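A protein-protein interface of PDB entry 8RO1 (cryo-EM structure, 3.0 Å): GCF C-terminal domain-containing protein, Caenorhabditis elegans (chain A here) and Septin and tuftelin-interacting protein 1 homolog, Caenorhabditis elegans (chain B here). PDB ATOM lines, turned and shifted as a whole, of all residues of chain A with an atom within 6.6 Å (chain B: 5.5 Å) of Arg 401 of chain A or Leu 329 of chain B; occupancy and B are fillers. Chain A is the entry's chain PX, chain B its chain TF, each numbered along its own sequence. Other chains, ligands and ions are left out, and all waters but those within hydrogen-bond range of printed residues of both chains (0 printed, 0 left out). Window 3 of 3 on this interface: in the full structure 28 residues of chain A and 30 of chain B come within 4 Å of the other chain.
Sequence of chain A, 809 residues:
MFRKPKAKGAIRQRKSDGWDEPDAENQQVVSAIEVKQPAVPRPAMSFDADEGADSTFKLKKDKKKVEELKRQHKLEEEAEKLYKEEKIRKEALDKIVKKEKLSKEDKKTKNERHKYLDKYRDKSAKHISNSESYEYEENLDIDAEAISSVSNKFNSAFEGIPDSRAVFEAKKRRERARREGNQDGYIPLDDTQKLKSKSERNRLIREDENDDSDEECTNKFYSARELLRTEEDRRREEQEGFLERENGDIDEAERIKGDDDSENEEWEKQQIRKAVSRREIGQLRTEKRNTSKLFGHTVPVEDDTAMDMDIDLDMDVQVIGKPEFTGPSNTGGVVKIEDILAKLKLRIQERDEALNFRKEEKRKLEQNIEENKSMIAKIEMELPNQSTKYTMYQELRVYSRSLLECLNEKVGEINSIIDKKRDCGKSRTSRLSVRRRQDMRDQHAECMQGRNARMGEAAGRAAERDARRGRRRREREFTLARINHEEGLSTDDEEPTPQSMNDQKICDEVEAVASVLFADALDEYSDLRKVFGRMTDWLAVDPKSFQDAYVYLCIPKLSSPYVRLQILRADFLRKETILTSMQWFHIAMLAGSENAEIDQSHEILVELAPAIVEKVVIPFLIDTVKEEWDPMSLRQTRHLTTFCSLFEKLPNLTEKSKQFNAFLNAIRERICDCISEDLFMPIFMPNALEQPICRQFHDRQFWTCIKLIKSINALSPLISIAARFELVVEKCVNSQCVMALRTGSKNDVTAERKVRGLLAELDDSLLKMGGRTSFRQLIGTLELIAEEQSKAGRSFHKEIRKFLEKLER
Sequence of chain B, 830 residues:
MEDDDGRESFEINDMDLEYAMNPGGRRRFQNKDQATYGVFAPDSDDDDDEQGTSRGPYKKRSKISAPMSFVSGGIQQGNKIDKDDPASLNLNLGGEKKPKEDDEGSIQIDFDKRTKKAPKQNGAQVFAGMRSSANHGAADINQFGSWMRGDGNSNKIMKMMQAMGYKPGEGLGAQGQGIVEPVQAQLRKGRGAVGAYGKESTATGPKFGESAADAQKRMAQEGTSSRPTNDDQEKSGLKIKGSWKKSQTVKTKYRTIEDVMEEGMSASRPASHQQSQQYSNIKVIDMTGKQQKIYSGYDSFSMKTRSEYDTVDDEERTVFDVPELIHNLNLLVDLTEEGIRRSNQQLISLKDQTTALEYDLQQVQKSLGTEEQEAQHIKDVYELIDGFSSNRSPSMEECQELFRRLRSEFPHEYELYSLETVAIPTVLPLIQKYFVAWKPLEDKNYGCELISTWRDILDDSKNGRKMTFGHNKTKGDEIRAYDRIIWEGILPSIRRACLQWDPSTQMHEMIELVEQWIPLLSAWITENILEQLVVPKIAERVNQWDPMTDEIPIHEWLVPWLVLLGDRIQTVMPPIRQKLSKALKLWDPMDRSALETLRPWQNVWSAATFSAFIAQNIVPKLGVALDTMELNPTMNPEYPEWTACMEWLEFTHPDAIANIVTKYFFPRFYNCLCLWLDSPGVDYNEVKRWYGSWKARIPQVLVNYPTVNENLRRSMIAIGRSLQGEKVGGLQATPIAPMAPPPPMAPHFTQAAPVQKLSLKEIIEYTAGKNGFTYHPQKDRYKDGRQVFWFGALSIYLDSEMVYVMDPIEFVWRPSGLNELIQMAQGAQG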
ATOM      1  N   LEU A 396      15.380 -12.758 -15.922  1.00  0.00           N
ATOM      2  CA  LEU A 396      15.107 -11.799 -16.983  1.00  0.00           C
ATOM      3  C   LEU A 396      14.858 -12.494 -18.310  1.00  0.00           C
ATOM      4  O   LEU A 396      14.018 -12.054 -19.104  1.00  0.00           O
ATOM      5  CB  LEU A 396      16.304 -10.869 -17.105  1.00  0.00           C
ATOM      6  CG  LEU A 396      16.371  -9.822 -18.207  1.00  0.00           C
ATOM      7  CD1 LEU A 396      15.390  -8.712 -17.919  1.00  0.00           C
ATOM      8  CD2 LEU A 396      17.806  -9.323 -18.305  1.00  0.00           C
ATOM      9  N   ARG A 397      15.610 -13.558 -18.574  1.00  0.00           N
ATOM     10  CA  ARG A 397      15.454 -14.315 -19.808  1.00  0.00           C
ATOM     11  C   ARG A 397      14.061 -14.923 -19.901  1.00  0.00           C
ATOM     12  O   ARG A 397      13.353 -14.739 -20.897  1.00  0.00           O
ATOM     13  CB  ARG A 397      16.555 -15.373 -19.857  1.00  0.00           C
ATOM     14  CG  ARG A 397      16.678 -16.212 -21.110  1.00  0.00           C
ATOM     15  CD  ARG A 397      17.685 -17.318 -20.840  1.00  0.00           C
ATOM     16  NE  ARG A 397      18.514 -17.599 -22.005  1.00  0.00           N
ATOM     17  CZ  ARG A 397      19.439 -18.549 -22.072  1.00  0.00           C
ATOM     18  NH1 ARG A 397      20.188 -18.643 -23.166  1.00  0.00           N
ATOM     19  NH2 ARG A 397      19.656 -19.387 -21.069  1.00  0.00           N
ATOM     20  N   VAL A 398      13.632 -15.615 -18.848  1.00  0.00           N
ATOM     21  CA  VAL A 398      12.321 -16.256 -18.858  1.00  0.00           C
ATOM     22  C   VAL A 398      11.212 -15.209 -18.849  1.00  0.00           C
ATOM     23  O   VAL A 398      10.230 -15.324 -19.593  1.00  0.00           O
ATOM     24  CB  VAL A 398      12.198 -17.226 -17.665  1.00  0.00           C
ATOM     25  CG1 VAL A 398      10.772 -17.838 -17.587  1.00  0.00           C
ATOM     26  CG2 VAL A 398      13.274 -18.318 -17.762  1.00  0.00           C
ATOM     27  N   TYR A 399      11.345 -14.176 -18.012  1.00  0.00           N
ATOM     28  CA  TYR A 399      10.313 -13.144 -17.929  1.00  0.00           C
ATOM     29  C   TYR A 399      10.130 -12.395 -19.244  1.00  0.00           C
ATOM     30  O   TYR A 399       9.003 -12.243 -19.731  1.00  0.00           O
ATOM     31  CB  TYR A 399      10.649 -12.144 -16.820  1.00  0.00           C
ATOM     32  CG  TYR A 399       9.664 -10.997 -16.784  1.00  0.00           C
ATOM     33  CD1 TYR A 399       8.394 -11.174 -16.254  1.00  0.00           C
ATOM     34  CD2 TYR A 399       9.993  -9.745 -17.291  1.00  0.00           C
ATOM     35  CE1 TYR A 399       7.481 -10.142 -16.225  1.00  0.00           C
ATOM     36  CE2 TYR A 399       9.080  -8.707 -17.273  1.00  0.00           C
ATOM     37  CZ  TYR A 399       7.825  -8.913 -16.740  1.00  0.00           C
ATOM     38  OH  TYR A 399       6.907  -7.892 -16.708  1.00  0.00           O
ATOM     39  N   SER A 400      11.223 -11.920 -19.837  1.00  0.00           N
ATOM     40  CA  SER A 400      11.107 -11.127 -21.058  1.00  0.00           C
ATOM     41  C   SER A 400      10.594 -11.962 -22.226  1.00  0.00           C
ATOM     42  O   SER A 400       9.849 -11.458 -23.072  1.00  0.00           O
ATOM     43  CB  SER A 400      12.457 -10.490 -21.393  1.00  0.00           C
ATOM     44  OG  SER A 400      13.471 -11.465 -21.533  1.00  0.00           O
ATOM     45  N   ARG A 401      10.983 -13.233 -22.292  1.00  0.00           N
ATOM     46  CA  ARG A 401      10.428 -14.125 -23.304  1.00  0.00           C
ATOM     47  C   ARG A 401       8.937 -14.360 -23.096  1.00  0.00           C
ATOM     48  O   ARG A 401       8.153 -14.290 -24.049  1.00  0.00           O
ATOM     49  CB  ARG A 401      11.168 -15.462 -23.269  1.00  0.00           C
ATOM     50  CG  ARG A 401      12.569 -15.430 -23.857  1.00  0.00           C
ATOM     51  CD  ARG A 401      13.167 -16.829 -23.907  1.00  0.00           C
ATOM     52  NE  ARG A 401      14.624 -16.796 -23.923  1.00  0.00           N
ATOM     53  CZ  ARG A 401      15.379 -16.306 -24.898  1.00  0.00           C
ATOM     54  NH1 ARG A 401      16.699 -16.291 -24.745  1.00  0.00           N
ATOM     55  NH2 ARG A 401      14.855 -15.823 -26.015  1.00  0.00           N
ATOM     56  N   SER A 402       8.524 -14.608 -21.852  1.00  0.00           N
ATOM     57  CA  SER A 402       7.115 -14.867 -21.565  1.00  0.00           C
ATOM     58  C   SER A 402       6.256 -13.629 -21.782  1.00  0.00           C
ATOM     59  O   SER A 402       5.116 -13.736 -22.250  1.00  0.00           O
ATOM     60  CB  SER A 402       6.960 -15.376 -20.131  1.00  0.00           C
ATOM     61  OG  SER A 402       7.713 -16.557 -19.920  1.00  0.00           O
ATOM     62  N   LEU A 403       6.776 -12.453 -21.445  1.00  0.00           N
ATOM     63  CA  LEU A 403       6.032 -11.223 -21.691  1.00  0.00           C
ATOM     64  C   LEU A 403       5.834 -11.000 -23.185  1.00  0.00           C
ATOM     65  O   LEU A 403       4.722 -10.710 -23.640  1.00  0.00           O
ATOM     66  CB  LEU A 403       6.775 -10.048 -21.058  1.00  0.00           C
ATOM     67  CG  LEU A 403       6.236  -8.634 -21.276  1.00  0.00           C
ATOM     68  CD1 LEU A 403       4.848  -8.476 -20.683  1.00  0.00           C
ATOM     69  CD2 LEU A 403       7.195  -7.639 -20.659  1.00  0.00           C
ATOM     70  N   LEU A 404       6.897 -11.166 -23.971  1.00  0.00           N
ATOM     71  CA  LEU A 404       6.768 -11.002 -25.412  1.00  0.00           C
ATOM     72  C   LEU A 404       5.900 -12.098 -26.009  1.00  0.00           C
ATOM     73  O   LEU A 404       5.154 -11.841 -26.959  1.00  0.00           O
ATOM     74  CB  LEU A 404       8.152 -10.991 -26.058  1.00  0.00           C
ATOM     75  CG  LEU A 404       8.984  -9.716 -25.874  1.00  0.00           C
ATOM     76  CD1 LEU A 404      10.400  -9.926 -26.385  1.00  0.00           C
ATOM     77  CD2 LEU A 404       8.343  -8.533 -26.593  1.00  0.00           C
ATOM     78  N   GLU A 405       5.948 -13.303 -25.439  1.00  0.00           N
ATOM     79  CA  GLU A 405       5.060 -14.372 -25.888  1.00  0.00           C
ATOM     80  C   GLU A 405       3.601 -14.014 -25.646  1.00  0.00           C
ATOM     81  O   GLU A 405       2.760 -14.140 -26.544  1.00  0.00           O
ATOM     82  CB  GLU A 405       5.400 -15.660 -25.139  1.00  0.00           C
ATOM     83  CG  GLU A 405       4.601 -16.884 -25.561  1.00  0.00           C
ATOM     84  CD  GLU A 405       5.095 -18.140 -24.884  1.00  0.00           C
ATOM     85  OE1 GLU A 405       5.940 -18.021 -23.972  1.00  0.00           O
ATOM     86  OE2 GLU A 405       4.638 -19.242 -25.253  1.00  0.00           O
ATOM     87  N   CYS A 406       3.284 -13.558 -24.434  1.00  0.00           N
ATOM     88  CA  CYS A 406       1.933 -13.093 -24.145  1.00  0.00           C
ATOM     89  C   CYS A 406       1.572 -11.904 -25.019  1.00  0.00           C
ATOM     90  O   CYS A 406       0.506 -11.875 -25.645  1.00  0.00           O
ATOM     91  CB  CYS A 406       1.806 -12.731 -22.663  1.00  0.00           C
ATOM     92  SG  CYS A 406       0.164 -12.125 -22.170  1.00  0.00           S
ATOM     93  N   ASN A 408       2.773 -11.068 -27.872  1.00  0.00           N
ATOM     94  CA  ASN A 408       2.616 -11.445 -29.270  1.00  0.00           C
ATOM     95  C   ASN A 408       1.188 -11.882 -29.555  1.00  0.00           C
ATOM     96  O   ASN A 408       0.631 -11.568 -30.613  1.00  0.00           O
ATOM     97  CB  ASN A 408       3.590 -12.565 -29.624  1.00  0.00           C
ATOM     98  CG  ASN A 408       4.993 -12.062 -29.884  1.00  0.00           C
ATOM     99  OD1 ASN A 408       5.196 -10.924 -30.311  1.00  0.00           O
ATOM    100  ND2 ASN A 408       5.977 -12.911 -29.615  1.00  0.00           N
ATOM    101  N   TYR A 525       2.283  -9.290 -16.499  1.00  0.00           N
ATOM    102  CA  TYR A 525       2.260  -8.994 -17.926  1.00  0.00           C
ATOM    103  C   TYR A 525       1.205  -7.968 -18.303  1.00  0.00           C
ATOM    104  O   TYR A 525       1.344  -7.329 -19.347  1.00  0.00           O
ATOM    105  CB  TYR A 525       2.002 -10.262 -18.760  1.00  0.00           C
ATOM    106  CG  TYR A 525       2.837 -11.477 -18.412  1.00  0.00           C
ATOM    107  CD1 TYR A 525       4.222 -11.431 -18.467  1.00  0.00           C
ATOM    108  CD2 TYR A 525       2.238 -12.677 -18.055  1.00  0.00           C
ATOM    109  CE1 TYR A 525       4.985 -12.541 -18.166  1.00  0.00           C
ATOM    110  CE2 TYR A 525       2.994 -13.791 -17.748  1.00  0.00           C
ATOM    111  CZ  TYR A 525       4.367 -13.719 -17.809  1.00  0.00           C
ATOM    112  OH  TYR A 525       5.132 -14.822 -17.503  1.00  0.00           O
ATOM    113  N   TRP A 538      16.963  -4.545 -13.812  1.00  0.00           N
ATOM    114  CA  TRP A 538      18.155  -4.800 -14.609  1.00  0.00           C
ATOM    115  C   TRP A 538      19.054  -3.570 -14.659  1.00  0.00           C
ATOM    116  O   TRP A 538      20.278  -3.681 -14.529  1.00  0.00           O
ATOM    117  CB  TRP A 538      17.691  -5.240 -15.995  1.00  0.00           C
ATOM    118  CG  TRP A 538      18.712  -5.655 -16.979  1.00  0.00           C
ATOM    119  CD1 TRP A 538      20.044  -5.872 -16.776  1.00  0.00           C
ATOM    120  CD2 TRP A 538      18.457  -5.963 -18.348  1.00  0.00           C
ATOM    121  NE1 TRP A 538      20.640  -6.261 -17.950  1.00  0.00           N
ATOM    122  CE2 TRP A 538      19.684  -6.333 -18.929  1.00  0.00           C
ATOM    123  CE3 TRP A 538      17.306  -5.945 -19.146  1.00  0.00           C
ATOM    124  CZ2 TRP A 538      19.793  -6.689 -20.270  1.00  0.00           C
ATOM    125  CZ3 TRP A 538      17.411  -6.310 -20.474  1.00  0.00           C
ATOM    126  CH2 TRP A 538      18.649  -6.673 -21.026  1.00  0.00           C
ATOM    127  N   LEU B 325      16.061  -7.974 -31.822  1.00  0.00           N
ATOM    128  CA  LEU B 325      15.486  -7.915 -30.486  1.00  0.00           C
ATOM    129  C   LEU B 325      15.755  -9.211 -29.734  1.00  0.00           C
ATOM    130  O   LEU B 325      16.407  -9.222 -28.693  1.00  0.00           O
ATOM    131  CB  LEU B 325      13.981  -7.647 -30.574  1.00  0.00           C
ATOM    132  CG  LEU B 325      13.182  -7.563 -29.271  1.00  0.00           C
ATOM    133  CD1 LEU B 325      13.717  -6.467 -28.366  1.00  0.00           C
ATOM    134  CD2 LEU B 325      11.716  -7.323 -29.588  1.00  0.00           C
ATOM    135  N   ILE B 326      15.240 -10.310 -30.284  1.00  0.00           N
ATOM    136  CA  ILE B 326      15.386 -11.608 -29.634  1.00  0.00           C
ATOM    137  C   ILE B 326      16.836 -12.076 -29.704  1.00  0.00           C
ATOM    138  O   ILE B 326      17.297 -12.820 -28.828  1.00  0.00           O
ATOM    139  CB  ILE B 326      14.427 -12.641 -30.267  1.00  0.00           C
ATOM    140  CG1 ILE B 326      12.955 -12.204 -30.136  1.00  0.00           C
ATOM    141  CG2 ILE B 326      14.624 -14.029 -29.634  1.00  0.00           C
ATOM    142  CD1 ILE B 326      12.410 -12.087 -28.704  1.00  0.00           C
ATOM    143  N   HIS B 327      17.574 -11.660 -30.740  1.00  0.00           N
ATOM    144  CA  HIS B 327      18.984 -12.030 -30.851  1.00  0.00           C
ATOM    145  C   HIS B 327      19.799 -11.465 -29.694  1.00  0.00           C
ATOM    146  O   HIS B 327      20.685 -12.145 -29.162  1.00  0.00           O
ATOM    147  CB  HIS B 327      19.561 -11.585 -32.209  1.00  0.00           C
ATOM    148  CG  HIS B 327      19.482 -10.110 -32.487  1.00  0.00           C
ATOM    149  ND1 HIS B 327      20.280  -9.181 -31.853  1.00  0.00           N
ATOM    150  CD2 HIS B 327      18.697  -9.407 -33.339  1.00  0.00           C
ATOM    151  CE1 HIS B 327      19.990  -7.972 -32.299  1.00  0.00           C
ATOM    152  NE2 HIS B 327      19.031  -8.082 -33.201  1.00  0.00           N
ATOM    153  N   ASN B 328      19.511 -10.234 -29.280  1.00  0.00           N
ATOM    154  CA  ASN B 328      20.265  -9.651 -28.181  1.00  0.00           C
ATOM    155  C   ASN B 328      19.955 -10.331 -26.858  1.00  0.00           C
ATOM    156  O   ASN B 328      20.840 -10.445 -26.003  1.00  0.00           O
ATOM    157  CB  ASN B 328      19.968  -8.158 -28.088  1.00  0.00           C
ATOM    158  CG  ASN B 328      20.876  -7.443 -27.115  1.00  0.00           C
ATOM    159  OD1 ASN B 328      20.399  -6.748 -26.224  1.00  0.00           O
ATOM    160  ND2 ASN B 328      22.185  -7.595 -27.281  1.00  0.00           N
ATOM    161  N   LEU B 329      18.716 -10.785 -26.665  1.00  0.00           N
ATOM    162  CA  LEU B 329      18.400 -11.507 -25.440  1.00  0.00           C
ATOM    163  C   LEU B 329      19.106 -12.856 -25.393  1.00  0.00           C
ATOM    164  O   LEU B 329      19.615 -13.259 -24.343  1.00  0.00           O
ATOM    165  CB  LEU B 329      16.889 -11.702 -25.336  1.00  0.00           C
ATOM    166  CG  LEU B 329      16.326 -12.054 -23.958  1.00  0.00           C
ATOM    167  CD1 LEU B 329      16.282 -10.833 -23.051  1.00  0.00           C
ATOM    168  CD2 LEU B 329      14.944 -12.681 -24.099  1.00  0.00           C
ATOM    169  N   ASN B 330      19.146 -13.564 -26.521  1.00  0.00           N
ATOM    170  CA  ASN B 330      19.826 -14.854 -26.563  1.00  0.00           C
ATOM    171  C   ASN B 330      21.332 -14.700 -26.391  1.00  0.00           C
ATOM    172  O   ASN B 330      21.947 -15.350 -25.538  1.00  0.00           O
ATOM    173  CB  ASN B 330      19.520 -15.556 -27.887  1.00  0.00           C
ATOM    174  CG  ASN B 330      18.060 -15.935 -28.023  1.00  0.00           C
ATOM    175  OD1 ASN B 330      17.288 -15.804 -27.081  1.00  0.00           O
ATOM    176  ND2 ASN B 330      17.674 -16.406 -29.202  1.00  0.00           N
ATOM    177  N   LEU B 331      21.935 -13.819 -27.191  1.00  0.00           N
ATOM    178  CA  LEU B 331      23.381 -13.626 -27.180  1.00  0.00           C
ATOM    179  C   LEU B 331      23.911 -13.106 -25.847  1.00  0.00           C
ATOM    180  O   LEU B 331      25.043 -13.423 -25.465  1.00  0.00           O
ATOM    181  CB  LEU B 331      23.771 -12.662 -28.303  1.00  0.00           C
ATOM    182  CG  LEU B 331      23.670 -13.184 -29.741  1.00  0.00           C
ATOM    183  CD1 LEU B 331      23.831 -12.046 -30.730  1.00  0.00           C
ATOM    184  CD2 LEU B 331      24.690 -14.278 -30.033  1.00  0.00           C
ATOM    185  N   LEU B 332      23.120 -12.318 -25.127  1.00  0.00           N
ATOM    186  CA  LEU B 332      23.600 -11.776 -23.862  1.00  0.00           C
ATOM    187  C   LEU B 332      23.679 -12.822 -22.754  1.00  0.00           C
ATOM    188  O   LEU B 332      24.621 -12.798 -21.957  1.00  0.00           O
ATOM    189  CB  LEU B 332      22.695 -10.619 -23.432  1.00  0.00           C
ATOM    190  CG  LEU B 332      23.101  -9.792 -22.206  1.00  0.00           C
ATOM    191  CD1 LEU B 332      24.492  -9.182 -22.366  1.00  0.00           C
ATOM    192  CD2 LEU B 332      22.079  -8.707 -21.935  1.00  0.00           C
ATOM    193  N   VAL B 333      22.740 -13.770 -22.694  1.00  0.00           N
ATOM    194  CA  VAL B 333      22.841 -14.779 -21.634  1.00  0.00           C
ATOM    195  C   VAL B 333      23.979 -15.761 -21.890  1.00  0.00           C
ATOM    196  O   VAL B 333      24.635 -16.221 -20.947  1.00  0.00           O
ATOM    197  CB  VAL B 333      21.515 -15.553 -21.457  1.00  0.00           C
ATOM    198  CG1 VAL B 333      21.586 -16.444 -20.209  1.00  0.00           C
ATOM    199  CG2 VAL B 333      20.274 -14.625 -21.360  1.00  0.00           C
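The side-chain amide oxygen of Asn 330 of chain B lies within hydrogen-bond range of the guanidinium group of Arg 401 of chain A, at 2.5 Å.
O of Leu 396 of chain A is in hydrogen-bond range of OG of Ser 400 of chain A (2.6 Å).
O of Arg 397 of chain A is in hydrogen-bond range of OG of Ser 400 of chain A, 3.3 Å away.
O of Leu 404 of chain A sits close to ND2 of Asn 408 of chain A (3.0 Å).
O of Ile 326 of chain B lies close to OD1 of Asn 330 of chain B, 3.5 Å away.
Val 333 of chain B touches Arg 397 of chain A.
OG of Ser 400 of chain A touches CD2 of Leu 329 of chain B, 3.2 Å away.
Arg 401 of chain A touches Leu 329 of chain B (CG to CD2, 3.6 Å).
Leu 404 of chain A touches Ile 326 of chain B.
Trp 538 of chain A touches Leu 332 of chain B (CZ2 to CD2, 3.5 Å).
Of the printed residues of chain B, Ser 400 of chain A touches Leu 329.
Arg 401 of chain A touches just these residues of chain B: Leu 329 (3.6 Å) and Asn 330 (2.5 Å).
Of the printed residues of chain B, Trp 538 of chain A touches Leu 332 (3.5 Å).
Leu 325 of chain B touches none of the printed residues of chain A.
Asn 328 of chain B touches none of the printed residues of chain A.
Of chain A, only Ser 400 and Arg 401 come within 4 Å of Leu 329 of chain B.
Of the printed residues of chain A, Asn 330 of chain B touches Arg 401.
The nearest residue of chain A that does not touch Leu 329 of chain B is Arg 397 of chain A (4.1 Å).
Hydrophobic or aromatic side chains of chain A that line the printed part of chain B: Leu 404 and Trp 538.
Among the printed residues, no Asp or Glu carboxylate lies within 4 Å of a Lys or Arg side-chain nitrogen of the other chain.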
